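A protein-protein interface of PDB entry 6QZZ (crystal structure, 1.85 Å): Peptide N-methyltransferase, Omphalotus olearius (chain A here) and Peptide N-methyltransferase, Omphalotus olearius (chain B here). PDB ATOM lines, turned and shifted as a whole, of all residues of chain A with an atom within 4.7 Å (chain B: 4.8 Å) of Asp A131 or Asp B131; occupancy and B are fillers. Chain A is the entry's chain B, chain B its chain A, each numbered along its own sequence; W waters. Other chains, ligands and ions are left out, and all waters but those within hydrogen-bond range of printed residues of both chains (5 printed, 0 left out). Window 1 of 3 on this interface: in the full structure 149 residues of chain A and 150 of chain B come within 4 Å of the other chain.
A ring nitrogen (NE2) of His B99 sits at hydrogen-bond distance from the backbone carbonyl oxygen (O) of Asp A131.
NE2 of His A99 sits at hydrogen-bond distance from O of Asp B131 (2.8 Å).
The side-chain carboxylate of Asp B131 lies close to the side-chain carboxylate of Asp A131 (2.3 Å).
The backbone NH of His B99 sits at hydrogen-bond distance from the backbone carbonyl oxygen of Val B127, at 3.4 Å.
The side-chain hydroxyl of Ser B128 sits at hydrogen-bond distance from the backbone NH of Asp B131.
The backbone carbonyl oxygen (O) of Ser B128 sits at hydrogen-bond distance from the side-chain sulfur (SG) of Cys B132 (3.5 Å).
The backbone NH (N) of His A99 sits at hydrogen-bond distance from the backbone carbonyl oxygen (O) of Val A127 (3.4 Å).
The backbone NH of Asp A131 sits at hydrogen-bond distance from the side-chain hydroxyl of Ser A128 (2.9 Å).
The backbone carbonyl oxygen (O) of Ser A128 is in hydrogen-bond range of the side-chain sulfur (SG) of Cys A132 (3.5 Å).
Among the printed residues, merely in contact across the chains: Gly A126 with Asp B131 (3.5 Å), Asp A131 with Gly B126 (3.6 Å), Asp A131 with Pro B125 (3.6 Å), Pro A125 with Asp B131 (3.6 Å), Val A127 with Pro B125 (3.6 Å), Pro A125 with Val B127 (3.7 Å), Cys A132 with Pro B125 (3.8 Å), Pro A125 with Cys B132 (3.8 Å), Pro A125 with Ala B135 (3.9 Å), Ala A135 with Pro B125 (3.9 Å), Val A127 with Gly B126 (3.9 Å), Gly A126 with Val B127 (3.9 Å), Phe A134 with His B99 (3.95 Å) and His A99 with Phe B134 (3.96 Å).
Asp A131 touches just these residues of chain B: His B99, Pro B125, Gly B126 and Asp B131.
Of chain A, only His A99 (2.8 Å), Pro A125 (3.6 Å), Gly A126 (3.5 Å) and Asp A131 (2.3 Å) come within 4 Å of Asp B131.
Of the printed residues of chain A, Gly B126 touches Val A127 and Asp A131.
Printed residues of chain B within 4 Å of Val A127: Pro B125 and Gly B126.
Of the printed residues of chain B, Ala A135 touches Pro B125 (3.9 Å).
Of the printed residues of chain A, Pro B125 touches Val A127 (3.6 Å), Asp A131 (3.6 Å), Cys A132 (3.8 Å) and Ala A135 (3.9 Å).
Of the printed residues of chain B, Gly A126 touches Val B127 and Asp B131.
Ala A129 touches none of the printed residues of chain B.
The nearest residue of chain B that does not touch Asp A131 is Ser B128 (4.3 Å).
Hydrophobic or aromatic side chains of chain A within 4 Å of the printed part of chain B: His A99, Pro A125, Val A127, Phe A134 and Ala A135.
Of the 12 printed residues of chain B, 8 touch a printed residue of chain A.
Hydrophobic or aromatic side chains of chain B within 4 Å of the printed part of chain A: His B99, Pro B125, Val B127, Phe B134 and Ala B135.
Among the printed residues, no Asp or Glu carboxylate lies within 4 Å of a Lys or Arg side-chain nitrogen of the other chain.
Water W2 lies within hydrogen-bond range of the side-chain carboxylate (OE1) of Glu B130 and the side-chain carboxylate (OE2) of Glu A130.
Water W4 bridges the side-chain carboxylate (OE2) of Glu A130 (2.6 Å) and the side-chain carboxylate (OE1) of Glu B130 (2.7 Å).
Water W1 lies within hydrogen-bond range of OE2 of Glu A130 (2.6 Å) and OE1 of Glu B130 (3.3 Å).
Water W3 lies within hydrogen-bond range of the side-chain hydroxyl of Ser A128 (2.6 Å) and the side-chain carboxylate of Asp B131 (2.8 Å).
Water W5 bridges the side-chain hydroxyl (OG) of Ser B128 (2.6 Å) and the side-chain carboxylate (OD1) of Asp A131 (2.7 Å).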
ATOM      1  N   HIS A  99       8.790 -21.383 -17.641  1.00  0.00           N
ATOM      2  CA  HIS A  99       9.413 -21.999 -18.828  1.00  0.00           C
ATOM      3  C   HIS A  99       8.263 -22.493 -19.702  1.00  0.00           C
ATOM      4  O   HIS A  99       7.386 -23.221 -19.233  1.00  0.00           O
ATOM      5  CB  HIS A  99      10.359 -23.111 -18.374  1.00  0.00           C
ATOM      6  CG  HIS A  99      11.132 -23.799 -19.440  1.00  0.00           C
ATOM      7  ND1 HIS A  99      10.530 -24.315 -20.578  1.00  0.00           N
ATOM      8  CD2 HIS A  99      12.435 -24.170 -19.480  1.00  0.00           C
ATOM      9  CE1 HIS A  99      11.447 -24.923 -21.310  1.00  0.00           C
ATOM     10  NE2 HIS A  99      12.639 -24.872 -20.638  1.00  0.00           N
ATOM     11  N   PRO A 125      14.114 -21.278 -23.623  1.00  0.00           N
ATOM     12  CA  PRO A 125      13.904 -21.673 -22.242  1.00  0.00           C
ATOM     13  C   PRO A 125      13.582 -20.451 -21.377  1.00  0.00           C
ATOM     14  O   PRO A 125      13.958 -19.324 -21.719  1.00  0.00           O
ATOM     15  CB  PRO A 125      15.236 -22.336 -21.886  1.00  0.00           C
ATOM     16  CG  PRO A 125      16.232 -21.600 -22.749  1.00  0.00           C
ATOM     17  CD  PRO A 125      15.522 -21.388 -24.058  1.00  0.00           C
ATOM     18  N   GLY A 126      12.883 -20.699 -20.274  1.00  0.00           N
ATOM     19  CA  GLY A 126      12.596 -19.683 -19.262  1.00  0.00           C
ATOM     20  C   GLY A 126      12.775 -20.246 -17.875  1.00  0.00           C
ATOM     21  O   GLY A 126      13.111 -21.442 -17.741  1.00  0.00           O
ATOM     22  N   VAL A 127      12.639 -19.381 -16.888  1.00  0.00           N
ATOM     23  CA  VAL A 127      12.734 -19.748 -15.448  1.00  0.00           C
ATOM     24  C   VAL A 127      11.431 -20.445 -15.031  1.00  0.00           C
ATOM     25  O   VAL A 127      10.368 -19.810 -15.117  1.00  0.00           O
ATOM     26  CB  VAL A 127      12.992 -18.484 -14.615  1.00  0.00           C
ATOM     27  CG1 VAL A 127      12.843 -18.762 -13.128  1.00  0.00           C
ATOM     28  CG2 VAL A 127      14.344 -17.866 -14.945  1.00  0.00           C
ATOM     29  N   SER A 128      11.507 -21.705 -14.616  1.00  0.00           N
ATOM     30  CA  SER A 128      10.344 -22.522 -14.187  1.00  0.00           C
ATOM     31  C   SER A 128      10.064 -22.300 -12.701  1.00  0.00           C
ATOM     32  O   SER A 128      10.949 -21.767 -11.975  1.00  0.00           O
ATOM     33  CB  SER A 128      10.588 -23.969 -14.440  1.00  0.00           C
ATOM     34  OG  SER A 128      11.556 -24.458 -13.520  1.00  0.00           O
ATOM     35  N   ALA A 129       8.922 -22.792 -12.241  1.00  0.00           N
ATOM     36  CA  ALA A 129       8.575 -22.837 -10.809  1.00  0.00           C
ATOM     37  C   ALA A 129       9.601 -23.697 -10.060  1.00  0.00           C
ATOM     38  O   ALA A 129       9.870 -23.422  -8.871  1.00  0.00           O
ATOM     39  CB  ALA A 129       7.181 -23.345 -10.618  1.00  0.00           C
ATOM     40  N   GLU A 130      10.164 -24.706 -10.714  1.00  0.00           N
ATOM     41  CA  GLU A 130      11.188 -25.581 -10.091  1.00  0.00           C
ATOM     42  C   GLU A 130      12.507 -24.791  -9.939  1.00  0.00           C
ATOM     43  O   GLU A 130      13.152 -24.900  -8.891  1.00  0.00           O
ATOM     44  CB  GLU A 130      11.346 -26.863 -10.906  1.00  0.00           C
ATOM     45  CG  GLU A 130      12.390 -27.792 -10.335  1.00  0.00           C
ATOM     46  CD  GLU A 130      12.356 -29.174 -10.947  1.00  0.00           C
ATOM     47  OE1 GLU A 130      11.593 -29.989 -10.442  1.00  0.00           O
ATOM     48  OE2 GLU A 130      13.048 -29.400 -11.955  1.00  0.00           O
ATOM     49  N   ASP A 131      12.885 -23.999 -10.939  1.00  0.00           N
ATOM     50  CA  ASP A 131      14.031 -23.065 -10.852  1.00  0.00           C
ATOM     51  C   ASP A 131      13.830 -22.178  -9.627  1.00  0.00           C
ATOM     52  O   ASP A 131      14.794 -22.055  -8.838  1.00  0.00           O
ATOM     53  CB  ASP A 131      14.205 -22.242 -12.121  1.00  0.00           C
ATOM     54  CG  ASP A 131      14.737 -23.070 -13.261  1.00  0.00           C
ATOM     55  OD1 ASP A 131      15.492 -24.012 -12.981  1.00  0.00           O
ATOM     56  OD2 ASP A 131      14.400 -22.757 -14.419  1.00  0.00           O
ATOM     57  N   CYS A 132      12.623 -21.624  -9.453  1.00  0.00           N
ATOM     58  CA  CYS A 132      12.292 -20.761  -8.294  1.00  0.00           C
ATOM     59  C   CYS A 132      12.427 -21.569  -7.009  1.00  0.00           C
ATOM     60  O   CYS A 132      13.009 -21.041  -6.034  1.00  0.00           O
ATOM     61  CB  CYS A 132      10.912 -20.138  -8.403  1.00  0.00           C
ATOM     62  SG  CYS A 132      10.807 -18.982  -9.791  1.00  0.00           S
ATOM     63  N   LEU A 133      11.913 -22.791  -7.015  1.00  0.00           N
ATOM     64  CA  LEU A 133      11.944 -23.683  -5.837  1.00  0.00           C
ATOM     65  C   LEU A 133      13.400 -23.846  -5.372  1.00  0.00           C
ATOM     66  O   LEU A 133      13.665 -23.634  -4.161  1.00  0.00           O
ATOM     67  CB  LEU A 133      11.276 -25.006  -6.218  1.00  0.00           C
ATOM     68  CG  LEU A 133      11.026 -25.985  -5.081  1.00  0.00           C
ATOM     69  CD1 LEU A 133       9.859 -26.906  -5.407  1.00  0.00           C
ATOM     70  CD2 LEU A 133      12.285 -26.788  -4.797  1.00  0.00           C
ATOM     71  N   PHE A 134      14.321 -24.193  -6.271  1.00  0.00           N
ATOM     72  CA  PHE A 134      15.752 -24.407  -5.915  1.00  0.00           C
ATOM     73  C   PHE A 134      16.309 -23.151  -5.243  1.00  0.00           C
ATOM     74  O   PHE A 134      16.962 -23.248  -4.175  1.00  0.00           O
ATOM     75  CB  PHE A 134      16.569 -24.775  -7.152  1.00  0.00           C
ATOM     76  CG  PHE A 134      16.134 -26.034  -7.852  1.00  0.00           C
ATOM     77  CD1 PHE A 134      15.592 -27.098  -7.143  1.00  0.00           C
ATOM     78  CD2 PHE A 134      16.334 -26.182  -9.216  1.00  0.00           C
ATOM     79  CE1 PHE A 134      15.213 -28.260  -7.798  1.00  0.00           C
ATOM     80  CE2 PHE A 134      15.969 -27.350  -9.866  1.00  0.00           C
ATOM     81  CZ  PHE A 134      15.415 -28.386  -9.157  1.00  0.00           C
ATOM     82  N   ALA A 135      16.032 -21.991  -5.838  1.00  0.00           N
ATOM     83  CA  ALA A 135      16.526 -20.688  -5.359  1.00  0.00           C
ATOM     84  C   ALA A 135      15.955 -20.349  -3.975  1.00  0.00           C
ATOM     85  O   ALA A 135      16.737 -19.890  -3.116  1.00  0.00           O
ATOM     86  CB  ALA A 135      16.213 -19.630  -6.376  1.00  0.00           C
ATOM     87  N   HIS B  99      21.573 -21.299 -14.029  1.00  0.00           N
ATOM     88  CA  HIS B  99      20.925 -21.058 -12.724  1.00  0.00           C
ATOM     89  C   HIS B  99      22.022 -21.132 -11.663  1.00  0.00           C
ATOM     90  O   HIS B  99      22.776 -22.108 -11.604  1.00  0.00           O
ATOM     91  CB  HIS B  99      19.823 -22.093 -12.542  1.00  0.00           C
ATOM     92  CG  HIS B  99      18.989 -21.957 -11.322  1.00  0.00           C
ATOM     93  ND1 HIS B  99      19.547 -21.860 -10.058  1.00  0.00           N
ATOM     94  CD2 HIS B  99      17.651 -22.055 -11.151  1.00  0.00           C
ATOM     95  CE1 HIS B  99      18.584 -21.824  -9.161  1.00  0.00           C
ATOM     96  NE2 HIS B  99      17.399 -21.962  -9.805  1.00  0.00           N
ATOM     97  N   PRO B 125      16.540 -17.151  -9.370  1.00  0.00           N
ATOM     98  CA  PRO B 125      16.665 -18.260 -10.304  1.00  0.00           C
ATOM     99  C   PRO B 125      17.107 -17.781 -11.690  1.00  0.00           C
ATOM    100  O   PRO B 125      16.897 -16.624 -12.054  1.00  0.00           O
ATOM    101  CB  PRO B 125      15.244 -18.848 -10.319  1.00  0.00           C
ATOM    102  CG  PRO B 125      14.361 -17.631 -10.046  1.00  0.00           C
ATOM    103  CD  PRO B 125      15.137 -16.826  -9.032  1.00  0.00           C
ATOM    104  N   GLY B 126      17.734 -18.690 -12.428  1.00  0.00           N
ATOM    105  CA  GLY B 126      18.116 -18.477 -13.827  1.00  0.00           C
ATOM    106  C   GLY B 126      17.788 -19.681 -14.667  1.00  0.00           C
ATOM    107  O   GLY B 126      17.287 -20.693 -14.128  1.00  0.00           O
ATOM    108  N   VAL B 127      18.021 -19.537 -15.958  1.00  0.00           N
ATOM    109  CA  VAL B 127      17.818 -20.616 -16.959  1.00  0.00           C
ATOM    110  C   VAL B 127      18.985 -21.602 -16.856  1.00  0.00           C
ATOM    111  O   VAL B 127      20.135 -21.200 -17.094  1.00  0.00           O
ATOM    112  CB  VAL B 127      17.711 -19.998 -18.360  1.00  0.00           C
ATOM    113  CG1 VAL B 127      17.701 -21.068 -19.435  1.00  0.00           C
ATOM    114  CG2 VAL B 127      16.492 -19.086 -18.472  1.00  0.00           C
ATOM    115  N   SER B 128      18.697 -22.853 -16.517  1.00  0.00           N
ATOM    116  CA  SER B 128      19.705 -23.936 -16.382  1.00  0.00           C
ATOM    117  C   SER B 128      19.930 -24.613 -17.728  1.00  0.00           C
ATOM    118  O   SER B 128      19.098 -24.433 -18.649  1.00  0.00           O
ATOM    119  CB  SER B 128      19.257 -24.956 -15.385  1.00  0.00           C
ATOM    120  OG  SER B 128      18.180 -25.699 -15.927  1.00  0.00           O
ATOM    121  N   ALA B 129      20.971 -25.444 -17.792  1.00  0.00           N
ATOM    122  CA  ALA B 129      21.255 -26.312 -18.945  1.00  0.00           C
ATOM    123  C   ALA B 129      20.082 -27.277 -19.137  1.00  0.00           C
ATOM    124  O   ALA B 129      19.799 -27.654 -20.288  1.00  0.00           O
ATOM    125  CB  ALA B 129      22.552 -27.045 -18.735  1.00  0.00           C
ATOM    126  N   GLU B 130      19.412 -27.666 -18.053  1.00  0.00           N
ATOM    127  CA  GLU B 130      18.249 -28.587 -18.140  1.00  0.00           C
ATOM    128  C   GLU B 130      17.053 -27.840 -18.763  1.00  0.00           C
ATOM    129  O   GLU B 130      16.362 -28.423 -19.622  1.00  0.00           O
ATOM    130  CB  GLU B 130      17.925 -29.169 -16.765  1.00  0.00           C
ATOM    131  CG  GLU B 130      16.744 -30.116 -16.822  1.00  0.00           C
ATOM    132  CD  GLU B 130      16.569 -30.970 -15.588  1.00  0.00           C
ATOM    133  OE1 GLU B 130      16.060 -30.463 -14.587  1.00  0.00           O
ATOM    134  OE2 GLU B 130      16.911 -32.140 -15.664  1.00  0.00           O
ATOM    135  N   ASP B 131      16.842 -26.574 -18.390  1.00  0.00           N
ATOM    136  CA  ASP B 131      15.836 -25.689 -19.038  1.00  0.00           C
ATOM    137  C   ASP B 131      16.119 -25.660 -20.535  1.00  0.00           C
ATOM    138  O   ASP B 131      15.161 -25.862 -21.303  1.00  0.00           O
ATOM    139  CB  ASP B 131      15.823 -24.288 -18.454  1.00  0.00           C
ATOM    140  CG  ASP B 131      15.230 -24.262 -17.066  1.00  0.00           C
ATOM    141  OD1 ASP B 131      14.349 -25.103 -16.809  1.00  0.00           O
ATOM    142  OD2 ASP B 131      15.664 -23.404 -16.254  1.00  0.00           O
ATOM    143  N   CYS B 132      17.386 -25.475 -20.920  1.00  0.00           N
ATOM    144  CA  CYS B 132      17.796 -25.433 -22.349  1.00  0.00           C
ATOM    145  C   CYS B 132      17.489 -26.786 -22.980  1.00  0.00           C
ATOM    146  O   CYS B 132      16.958 -26.808 -24.102  1.00  0.00           O
ATOM    147  CB  CYS B 132      19.250 -25.043 -22.530  1.00  0.00           C
ATOM    148  SG  CYS B 132      19.564 -23.343 -21.991  1.00  0.00           S
ATOM    149  N   LEU B 133      17.818 -27.868 -22.277  1.00  0.00           N
ATOM    150  CA  LEU B 133      17.612 -29.241 -22.792  1.00  0.00           C
ATOM    151  C   LEU B 133      16.123 -29.425 -23.157  1.00  0.00           C
ATOM    152  O   LEU B 133      15.833 -29.864 -24.297  1.00  0.00           O
ATOM    153  CB  LEU B 133      18.105 -30.226 -21.734  1.00  0.00           C
ATOM    154  CG  LEU B 133      18.157 -31.688 -22.170  1.00  0.00           C
ATOM    155  CD1 LEU B 133      19.205 -32.440 -21.383  1.00  0.00           C
ATOM    156  CD2 LEU B 133      16.786 -32.330 -22.012  1.00  0.00           C
ATOM    157  N   PHE B 134      15.201 -29.108 -22.250  1.00  0.00           N
ATOM    158  CA  PHE B 134      13.737 -29.262 -22.502  1.00  0.00           C
ATOM    159  C   PHE B 134      13.343 -28.501 -23.776  1.00  0.00           C
ATOM    160  O   PHE B 134      12.631 -29.052 -24.640  1.00  0.00           O
ATOM    161  CB  PHE B 134      12.925 -28.769 -21.307  1.00  0.00           C
ATOM    162  CG  PHE B 134      13.191 -29.492 -20.013  1.00  0.00           C
ATOM    163  CD1 PHE B 134      13.546 -30.834 -19.998  1.00  0.00           C
ATOM    164  CD2 PHE B 134      13.030 -28.832 -18.804  1.00  0.00           C
ATOM    165  CE1 PHE B 134      13.768 -31.489 -18.798  1.00  0.00           C
ATOM    166  CE2 PHE B 134      13.239 -29.493 -17.602  1.00  0.00           C
ATOM    167  CZ  PHE B 134      13.601 -30.821 -17.606  1.00  0.00           C
ATOM    168  N   ALA B 135      13.826 -27.265 -23.906  1.00  0.00           N
ATOM    169  CA  ALA B 135      13.500 -26.368 -25.037  1.00  0.00           C
ATOM    170  C   ALA B 135      14.057 -26.919 -26.355  1.00  0.00           C
ATOM    171  O   ALA B 135      13.316 -26.896 -27.347  1.00  0.00           O
ATOM    172  CB  ALA B 135      14.009 -24.982 -24.769  1.00  0.00           C
HETATM  173  O   HOH W   1      12.942 -31.298 -13.750  1.00  0.00           O
HETATM  174  O   HOH W   2      15.669 -31.101 -12.114  1.00  0.00           O
HETATM  175  O   HOH W   3      12.860 -26.333 -14.842  1.00  0.00           O
HETATM  176  O   HOH W   4      14.579 -28.314 -13.746  1.00  0.00           O
HETATM  177  O   HOH W   5      16.627 -26.311 -13.877  1.00  0.00           O
